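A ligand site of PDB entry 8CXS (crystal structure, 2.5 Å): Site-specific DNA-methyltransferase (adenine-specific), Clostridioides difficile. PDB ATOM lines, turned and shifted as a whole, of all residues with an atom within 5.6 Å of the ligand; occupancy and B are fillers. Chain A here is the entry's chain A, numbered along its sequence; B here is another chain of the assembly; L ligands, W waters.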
ATOM      1  N   GLY A  29     -13.804  -4.702 -21.185  1.00  0.00           N
ATOM      2  CA  GLY A  29     -13.060  -4.056 -22.247  1.00  0.00           C
ATOM      3  C   GLY A  29     -12.555  -2.671 -21.925  1.00  0.00           C
ATOM      4  O   GLY A  29     -11.852  -2.072 -22.747  1.00  0.00           O
ATOM      5  N   ILE A  30     -12.873  -2.135 -20.742  1.00  0.00           N
ATOM      6  CA  ILE A  30     -12.444  -0.800 -20.331  1.00  0.00           C
ATOM      7  C   ILE A  30     -11.323  -0.949 -19.311  1.00  0.00           C
ATOM      8  O   ILE A  30     -11.458  -1.685 -18.333  1.00  0.00           O
ATOM      9  CB  ILE A  30     -13.618   0.006 -19.738  1.00  0.00           C
ATOM     10  CG1 ILE A  30     -14.930  -0.305 -20.467  1.00  0.00           C
ATOM     11  CG2 ILE A  30     -13.324   1.497 -19.786  1.00  0.00           C
ATOM     12  CD1 ILE A  30     -15.072   0.359 -21.817  1.00  0.00           C
ATOM     13  N   TYR A  31     -10.218  -0.263 -19.557  1.00  0.00           N
ATOM     14  CA  TYR A  31      -9.029  -0.332 -18.704  1.00  0.00           C
ATOM     15  C   TYR A  31      -8.734   1.038 -18.127  1.00  0.00           C
ATOM     16  O   TYR A  31      -8.733   2.035 -18.856  1.00  0.00           O
ATOM     17  CB  TYR A  31      -7.820  -0.861 -19.482  1.00  0.00           C
ATOM     18  CG  TYR A  31      -7.993  -2.278 -19.986  1.00  0.00           C
ATOM     19  CD1 TYR A  31      -8.550  -2.530 -21.238  1.00  0.00           C
ATOM     20  CD2 TYR A  31      -7.603  -3.364 -19.214  1.00  0.00           C
ATOM     21  CE1 TYR A  31      -8.714  -3.820 -21.699  1.00  0.00           C
ATOM     22  CE2 TYR A  31      -7.760  -4.659 -19.671  1.00  0.00           C
ATOM     23  CZ  TYR A  31      -8.315  -4.879 -20.918  1.00  0.00           C
ATOM     24  OH  TYR A  31      -8.472  -6.173 -21.375  1.00  0.00           O
ATOM     25  N   THR A  33      -6.258   3.652 -16.795  1.00  0.00           N
ATOM     26  CA  THR A  33      -4.856   4.063 -16.787  1.00  0.00           C
ATOM     27  C   THR A  33      -4.533   4.767 -15.466  1.00  0.00           C
ATOM     28  O   THR A  33      -5.334   5.564 -14.974  1.00  0.00           O
ATOM     29  CB  THR A  33      -4.573   5.005 -17.961  1.00  0.00           C
ATOM     30  OG1 THR A  33      -5.106   4.446 -19.161  1.00  0.00           O
ATOM     31  CG2 THR A  33      -3.075   5.211 -18.136  1.00  0.00           C
ATOM     32  N   ILE A  62      -9.074   9.034 -29.139  1.00  0.00           N
ATOM     33  CA  ILE A  62      -9.885   8.135 -29.953  1.00  0.00           C
ATOM     34  C   ILE A  62     -10.249   6.849 -29.242  1.00  0.00           C
ATOM     35  O   ILE A  62     -10.917   5.989 -29.835  1.00  0.00           O
ATOM     36  CB  ILE A  62      -9.205   7.745 -31.280  1.00  0.00           C
ATOM     37  CG1 ILE A  62      -7.829   7.136 -31.022  1.00  0.00           C
ATOM     38  CG2 ILE A  62      -9.078   8.943 -32.197  1.00  0.00           C
ATOM     39  CD1 ILE A  62      -7.206   6.596 -32.280  1.00  0.00           C
ATOM     40  N   SER A  63      -9.830   6.691 -27.991  1.00  0.00           N
ATOM     41  CA  SER A  63     -10.114   5.494 -27.202  1.00  0.00           C
ATOM     42  C   SER A  63     -10.445   5.888 -25.768  1.00  0.00           C
ATOM     43  O   SER A  63      -9.977   5.257 -24.810  1.00  0.00           O
ATOM     44  CB  SER A  63      -8.934   4.535 -27.244  1.00  0.00           C
ATOM     45  OG  SER A  63      -9.364   3.205 -27.071  1.00  0.00           O
ATOM     46  N   CYS A  64     -11.260   6.933 -25.611  1.00  0.00           N
ATOM     47  CA  CYS A  64     -11.310   7.669 -24.350  1.00  0.00           C
ATOM     48  C   CYS A  64     -11.879   6.867 -23.187  1.00  0.00           C
ATOM     49  O   CYS A  64     -11.587   7.194 -22.035  1.00  0.00           O
ATOM     50  CB  CYS A  64     -12.125   8.957 -24.533  1.00  0.00           C
ATOM     51  SG  CYS A  64     -13.822   8.672 -25.070  1.00  0.00           S
ATOM     52  N   GLY A  65     -12.671   5.834 -23.451  1.00  0.00           N
ATOM     53  CA  GLY A  65     -13.242   5.059 -22.361  1.00  0.00           C
ATOM     54  C   GLY A  65     -14.164   5.925 -21.529  1.00  0.00           C
ATOM     55  O   GLY A  65     -15.022   6.644 -22.055  1.00  0.00           O
ATOM     56  N   CYS A  66     -13.982   5.883 -20.205  1.00  0.00           N
ATOM     57  CA  CYS A  66     -14.774   6.701 -19.307  1.00  0.00           C
ATOM     58  C   CYS A  66     -14.251   8.130 -19.191  1.00  0.00           C
ATOM     59  O   CYS A  66     -14.884   8.945 -18.512  1.00  0.00           O
ATOM     60  CB  CYS A  66     -14.831   6.070 -17.913  1.00  0.00           C
ATOM     61  SG  CYS A  66     -15.879   4.610 -17.820  1.00  0.00           S
ATOM     62  N   ALA A 114     -13.682   9.678 -28.680  1.00  0.00           N
ATOM     63  CA  ALA A 114     -14.313   8.591 -29.428  1.00  0.00           C
ATOM     64  C   ALA A 114     -14.155   7.297 -28.659  1.00  0.00           C
ATOM     65  O   ALA A 114     -13.079   7.017 -28.107  1.00  0.00           O
ATOM     66  CB  ALA A 114     -13.717   8.448 -30.832  1.00  0.00           C
ATOM     67  N   ASP A 115     -15.218   6.499 -28.615  1.00  0.00           N
ATOM     68  CA  ASP A 115     -15.145   5.176 -28.024  1.00  0.00           C
ATOM     69  C   ASP A 115     -16.277   4.325 -28.582  1.00  0.00           C
ATOM     70  O   ASP A 115     -17.376   4.825 -28.846  1.00  0.00           O
ATOM     71  CB  ASP A 115     -15.215   5.218 -26.492  1.00  0.00           C
ATOM     72  CG  ASP A 115     -14.613   3.979 -25.852  1.00  0.00           C
ATOM     73  OD1 ASP A 115     -15.220   2.891 -25.960  1.00  0.00           O
ATOM     74  OD2 ASP A 115     -13.527   4.090 -25.245  1.00  0.00           O
ATOM     75  N   ILE A 116     -16.007   3.033 -28.751  1.00  0.00           N
ATOM     76  CA  ILE A 116     -16.998   2.101 -29.288  1.00  0.00           C
ATOM     77  C   ILE A 116     -18.053   1.712 -28.257  1.00  0.00           C
ATOM     78  O   ILE A 116     -19.018   1.017 -28.605  1.00  0.00           O
ATOM     79  CB  ILE A 116     -16.286   0.856 -29.849  1.00  0.00           C
ATOM     80  CG1 ILE A 116     -17.147   0.162 -30.904  1.00  0.00           C
ATOM     81  CG2 ILE A 116     -15.909  -0.103 -28.727  1.00  0.00           C
ATOM     82  CD1 ILE A 116     -16.461  -1.015 -31.565  1.00  0.00           C
ATOM     83  N   ASP A 117     -17.912   2.147 -27.007  1.00  0.00           N
ATOM     84  CA  ASP A 117     -18.782   1.727 -25.918  1.00  0.00           C
ATOM     85  C   ASP A 117     -19.759   2.857 -25.587  1.00  0.00           C
ATOM     86  O   ASP A 117     -19.348   3.925 -25.127  1.00  0.00           O
ATOM     87  CB  ASP A 117     -17.952   1.342 -24.698  1.00  0.00           C
ATOM     88  CG  ASP A 117     -18.774   0.747 -23.576  1.00  0.00           C
ATOM     89  OD1 ASP A 117     -19.456  -0.269 -23.808  1.00  0.00           O
ATOM     90  OD2 ASP A 117     -18.733   1.298 -22.452  1.00  0.00           O
ATOM     91  N   ALA A 120     -19.801   4.129 -21.834  1.00  0.00           N
ATOM     92  CA  ALA A 120     -18.645   4.947 -21.459  1.00  0.00           C
ATOM     93  C   ALA A 120     -18.792   6.370 -21.973  1.00  0.00           C
ATOM     94  O   ALA A 120     -18.491   7.333 -21.266  1.00  0.00           O
ATOM     95  CB  ALA A 120     -17.363   4.313 -21.982  1.00  0.00           C
ATOM     96  N   CYS A 149     -18.337   5.333 -31.892  1.00  0.00           N
ATOM     97  CA  CYS A 149     -18.023   4.778 -33.204  1.00  0.00           C
ATOM     98  C   CYS A 149     -16.795   3.893 -33.092  1.00  0.00           C
ATOM     99  O   CYS A 149     -16.121   3.858 -32.067  1.00  0.00           O
ATOM    100  CB  CYS A 149     -17.794   5.888 -34.228  1.00  0.00           C
ATOM    101  SG  CYS A 149     -16.319   6.882 -33.852  1.00  0.00           S
ATOM    102  N   ASP A 150     -16.521   3.170 -34.175  1.00  0.00           N
ATOM    103  CA  ASP A 150     -15.228   2.512 -34.357  1.00  0.00           C
ATOM    104  C   ASP A 150     -14.258   3.541 -34.894  1.00  0.00           C
ATOM    105  O   ASP A 150     -14.373   3.980 -36.046  1.00  0.00           O
ATOM    106  CB  ASP A 150     -15.377   1.323 -35.308  1.00  0.00           C
ATOM    107  CG  ASP A 150     -14.115   0.487 -35.402  1.00  0.00           C
ATOM    108  OD1 ASP A 150     -13.016   1.007 -35.109  1.00  0.00           O
ATOM    109  OD2 ASP A 150     -14.224  -0.692 -35.788  1.00  0.00           O
ATOM    110  N   SER A 151     -13.283   3.939 -34.069  1.00  0.00           N
ATOM    111  CA  SER A 151     -12.331   4.965 -34.484  1.00  0.00           C
ATOM    112  C   SER A 151     -11.556   4.579 -35.729  1.00  0.00           C
ATOM    113  O   SER A 151     -11.058   5.458 -36.440  1.00  0.00           O
ATOM    114  CB  SER A 151     -11.363   5.278 -33.347  1.00  0.00           C
ATOM    115  OG  SER A 151     -12.029   5.879 -32.252  1.00  0.00           O
ATOM    116  N   LEU A 152     -11.429   3.278 -36.014  1.00  0.00           N
ATOM    117  CA  LEU A 152     -10.735   2.822 -37.201  1.00  0.00           C
ATOM    118  C   LEU A 152     -11.611   2.852 -38.449  1.00  0.00           C
ATOM    119  O   LEU A 152     -11.097   2.598 -39.550  1.00  0.00           O
ATOM    120  CB  LEU A 152     -10.195   1.407 -36.983  1.00  0.00           C
ATOM    121  CG  LEU A 152      -9.213   1.235 -35.818  1.00  0.00           C
ATOM    122  CD1 LEU A 152      -8.620  -0.165 -35.822  1.00  0.00           C
ATOM    123  CD2 LEU A 152      -8.103   2.286 -35.866  1.00  0.00           C
ATOM    124  N   ASN A 166      -5.041   5.803 -24.598  1.00  0.00           N
ATOM    125  CA  ASN A 166      -4.627   4.423 -24.382  1.00  0.00           C
ATOM    126  C   ASN A 166      -5.483   3.536 -25.277  1.00  0.00           C
ATOM    127  O   ASN A 166      -6.662   3.291 -24.970  1.00  0.00           O
ATOM    128  CB  ASN A 166      -4.782   4.025 -22.915  1.00  0.00           C
ATOM    129  CG  ASN A 166      -4.386   2.588 -22.643  1.00  0.00           C
ATOM    130  OD1 ASN A 166      -3.648   1.979 -23.413  1.00  0.00           O
ATOM    131  ND2 ASN A 166      -4.865   2.039 -21.528  1.00  0.00           N
ATOM    132  N   PRO A 167      -4.937   3.065 -26.399  1.00  0.00           N
ATOM    133  CA  PRO A 167      -5.749   2.288 -27.363  1.00  0.00           C
ATOM    134  C   PRO A 167      -6.035   0.895 -26.842  1.00  0.00           C
ATOM    135  O   PRO A 167      -5.400   0.427 -25.884  1.00  0.00           O
ATOM    136  CB  PRO A 167      -4.856   2.238 -28.603  1.00  0.00           C
ATOM    137  CG  PRO A 167      -3.468   2.330 -28.061  1.00  0.00           C
ATOM    138  CD  PRO A 167      -3.550   3.229 -26.846  1.00  0.00           C
ATOM    139  N   PRO A 168      -6.999   0.188 -27.439  1.00  0.00           N
ATOM    140  CA  PRO A 168      -7.178  -1.234 -27.102  1.00  0.00           C
ATOM    141  C   PRO A 168      -6.045  -2.085 -27.654  1.00  0.00           C
ATOM    142  O   PRO A 168      -5.532  -1.837 -28.748  1.00  0.00           O
ATOM    143  CB  PRO A 168      -8.515  -1.582 -27.766  1.00  0.00           C
ATOM    144  CG  PRO A 168      -8.602  -0.640 -28.913  1.00  0.00           C
ATOM    145  CD  PRO A 168      -7.982   0.646 -28.429  1.00  0.00           C
ATOM    146  N   TYR A 179     -13.280  -8.965 -38.695  1.00  0.00           N
ATOM    147  CA  TYR A 179     -12.622  -7.696 -38.421  1.00  0.00           C
ATOM    148  C   TYR A 179     -11.183  -7.716 -38.909  1.00  0.00           C
ATOM    149  O   TYR A 179     -10.678  -6.709 -39.417  1.00  0.00           O
ATOM    150  CB  TYR A 179     -12.687  -7.382 -36.935  1.00  0.00           C
ATOM    151  CG  TYR A 179     -12.486  -5.916 -36.630  1.00  0.00           C
ATOM    152  CD1 TYR A 179     -13.552  -5.028 -36.659  1.00  0.00           C
ATOM    153  CD2 TYR A 179     -11.226  -5.425 -36.321  1.00  0.00           C
ATOM    154  CE1 TYR A 179     -13.372  -3.686 -36.393  1.00  0.00           C
ATOM    155  CE2 TYR A 179     -11.036  -4.079 -36.046  1.00  0.00           C
ATOM    156  CZ  TYR A 179     -12.117  -3.219 -36.077  1.00  0.00           C
ATOM    157  OH  TYR A 179     -11.941  -1.886 -35.814  1.00  0.00           O
ATOM    158  N   LEU A 197      -3.930  -5.153 -32.711  1.00  0.00           N
ATOM    159  CA  LEU A 197      -4.907  -4.118 -33.059  1.00  0.00           C
ATOM    160  C   LEU A 197      -4.340  -2.717 -32.815  1.00  0.00           C
ATOM    161  O   LEU A 197      -4.605  -1.795 -33.597  1.00  0.00           O
ATOM    162  CB  LEU A 197      -6.189  -4.319 -32.265  1.00  0.00           C
ATOM    163  CG  LEU A 197      -7.246  -3.208 -32.367  1.00  0.00           C
ATOM    164  CD1 LEU A 197      -7.714  -3.046 -33.802  1.00  0.00           C
ATOM    165  CD2 LEU A 197      -8.415  -3.483 -31.446  1.00  0.00           C
ATOM    166  N   PHE A 201      -4.171   1.694 -34.429  1.00  0.00           N
ATOM    167  CA  PHE A 201      -4.420   2.947 -33.727  1.00  0.00           C
ATOM    168  C   PHE A 201      -3.226   3.884 -33.823  1.00  0.00           C
ATOM    169  O   PHE A 201      -3.402   5.102 -33.917  1.00  0.00           O
ATOM    170  CB  PHE A 201      -4.790   2.675 -32.270  1.00  0.00           C
ATOM    171  CG  PHE A 201      -6.235   2.300 -32.083  1.00  0.00           C
ATOM    172  CD1 PHE A 201      -6.692   1.031 -32.434  1.00  0.00           C
ATOM    173  CD2 PHE A 201      -7.144   3.208 -31.573  1.00  0.00           C
ATOM    174  CE1 PHE A 201      -8.019   0.684 -32.257  1.00  0.00           C
ATOM    175  CE2 PHE A 201      -8.467   2.870 -31.393  1.00  0.00           C
ATOM    176  CZ  PHE A 201      -8.908   1.606 -31.743  1.00  0.00           C
ATOM    177  P    DA B   8      -2.337 -10.765 -24.952  1.00  0.00           P
ATOM    178  OP1  DA B   8      -3.337 -11.843 -24.752  1.00  0.00           O
ATOM    179  OP2  DA B   8      -2.355  -9.923 -26.170  1.00  0.00           O
ATOM    180  O5'  DA B   8      -2.384  -9.810 -23.681  1.00  0.00           O
ATOM    181  C5'  DA B   8      -2.873  -8.484 -23.795  1.00  0.00           C
ATOM    182  C4'  DA B   8      -3.191  -7.937 -22.425  1.00  0.00           C
ATOM    183  O4'  DA B   8      -3.388  -6.501 -22.513  1.00  0.00           O
ATOM    184  C3'  DA B   8      -4.448  -8.502 -21.769  1.00  0.00           C
ATOM    185  O3'  DA B   8      -4.193  -8.754 -20.399  1.00  0.00           O
ATOM    186  C2'  DA B   8      -5.467  -7.374 -21.954  1.00  0.00           C
ATOM    187  C1'  DA B   8      -4.562  -6.159 -21.814  1.00  0.00           C
ATOM    188  N9   DA B   8      -5.105  -4.938 -22.399  1.00  0.00           N
ATOM    189  C8   DA B   8      -5.851  -4.823 -23.545  1.00  0.00           C
ATOM    190  N7   DA B   8      -6.178  -3.583 -23.834  1.00  0.00           N
ATOM    191  C5   DA B   8      -5.617  -2.838 -22.808  1.00  0.00           C
ATOM    192  C6   DA B   8      -5.603  -1.450 -22.535  1.00  0.00           C
ATOM    193  N6   DA B   8      -6.208  -0.544 -23.307  1.00  0.00           N
ATOM    194  N1   DA B   8      -4.944  -1.037 -21.430  1.00  0.00           N
ATOM    195  C2   DA B   8      -4.342  -1.952 -20.661  1.00  0.00           C
ATOM    196  N3   DA B   8      -4.288  -3.273 -20.816  1.00  0.00           N
ATOM    197  C4   DA B   8      -4.955  -3.659 -21.925  1.00  0.00           C
HETATM  198  C1  LIG L   1      -8.969   3.034 -22.694  1.00  0.00           C
HETATM  199  S1  LIG L   1      -9.052   1.240 -22.669  1.00  0.00           S
HETATM  200  C2  LIG L   1      -9.493   0.885 -24.380  1.00  0.00           C
HETATM  201  C3  LIG L   1     -10.794   1.531 -24.815  1.00  0.00           C
HETATM  202  O1  LIG L   1     -10.850   1.424 -26.259  1.00  0.00           O
HETATM  203  C4  LIG L   1     -12.768   0.324 -25.540  1.00  0.00           C
HETATM  204  O2  LIG L   1     -14.185   0.456 -25.484  1.00  0.00           O
HETATM  205  C5  LIG L   1     -12.068   0.869 -24.280  1.00  0.00           C
HETATM  206  O3  LIG L   1     -12.852   1.820 -23.575  1.00  0.00           O
HETATM  207  C6  LIG L   1     -12.203   1.233 -26.622  1.00  0.00           C
HETATM  208  N1  LIG L   1     -12.250   0.673 -27.963  1.00  0.00           N
HETATM  209  C7  LIG L   1     -12.076  -0.639 -28.327  1.00  0.00           C
HETATM  210  N2  LIG L   1     -12.119  -0.848 -29.621  1.00  0.00           N
HETATM  211  C8  LIG L   1     -12.326   0.420 -30.143  1.00  0.00           C
HETATM  212  C9  LIG L   1     -12.467   0.886 -31.472  1.00  0.00           C
HETATM  213  N3  LIG L   1     -12.367   0.102 -32.552  1.00  0.00           N
HETATM  214  N4  LIG L   1     -12.687   2.205 -31.650  1.00  0.00           N
HETATM  215  C10 LIG L   1     -12.748   3.001 -30.578  1.00  0.00           C
HETATM  216  N5  LIG L   1     -12.631   2.671 -29.292  1.00  0.00           N
HETATM  217  C11 LIG L   1     -12.414   1.362 -29.140  1.00  0.00           C
HETATM  218  O   HOH W   1      -8.687   6.078 -21.390  1.00  0.00           O
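The side-chain hydroxyl of Ser 63 sits at hydrogen-bond distance from an oxygen (O1) of the ligand (2.5 Å).
N of Tyr 31 lies close to S1 of the ligand (3.6 Å).
O2 of the ligand sits at hydrogen-bond distance from OD1 of Asp 115 (2.7 Å).
The backbone NH of Ile 116 sits at hydrogen-bond distance from a nitrogen (N5) of the ligand, 3.4 Å away.
N of Ser 151 lies within hydrogen-bond range of N4 of the ligand, 3.0 Å away.
OD1 of Asp 150 sits at hydrogen-bond distance from N3 of the ligand.
O of Cys 149 sits close to N of Ile 116.
The side-chain hydroxyl (OG) of Ser 151 sits at hydrogen-bond distance from the backbone carbonyl oxygen (O) of Ile 62.
N of Asp 117 is in hydrogen-bond range of OD1 of Asp 115, at 3.0 Å.
O of Asp 115 is in hydrogen-bond range of N of Cys 149.
The side-chain carboxylate (OD1) of Asp 150 lies within hydrogen-bond range of the backbone NH (N) of Leu 152 (2.9 Å).
O of Asn 166 is in hydrogen-bond range of OG of Ser 63 (3.4 Å).
The backbone NH of Ser 63 sits at hydrogen-bond distance from the backbone carbonyl oxygen of Ala 114.
N of Gly 65 is in hydrogen-bond range of OD2 of Asp 115 (2.6 Å).
S1 of the ligand lies close to N6 of DA 8 of chain B.
Merely in contact with the ligand: Ile 30, Asn 166, Gly 29, Gly 65, Pro 168, Ile 62, Phe 201, Cys 149, Tyr 179 and Asp 117.
Within 4 Å of the ligand: Gly 29, Ile 30, Tyr 31, Ile 62, Ser 63, Gly 65, Asp 115, Ile 116, Asp 117, Cys 149, Asp 150, Ser 151, Asn 166, Pro 168, Tyr 179, Phe 201 and DA 8 of chain B.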
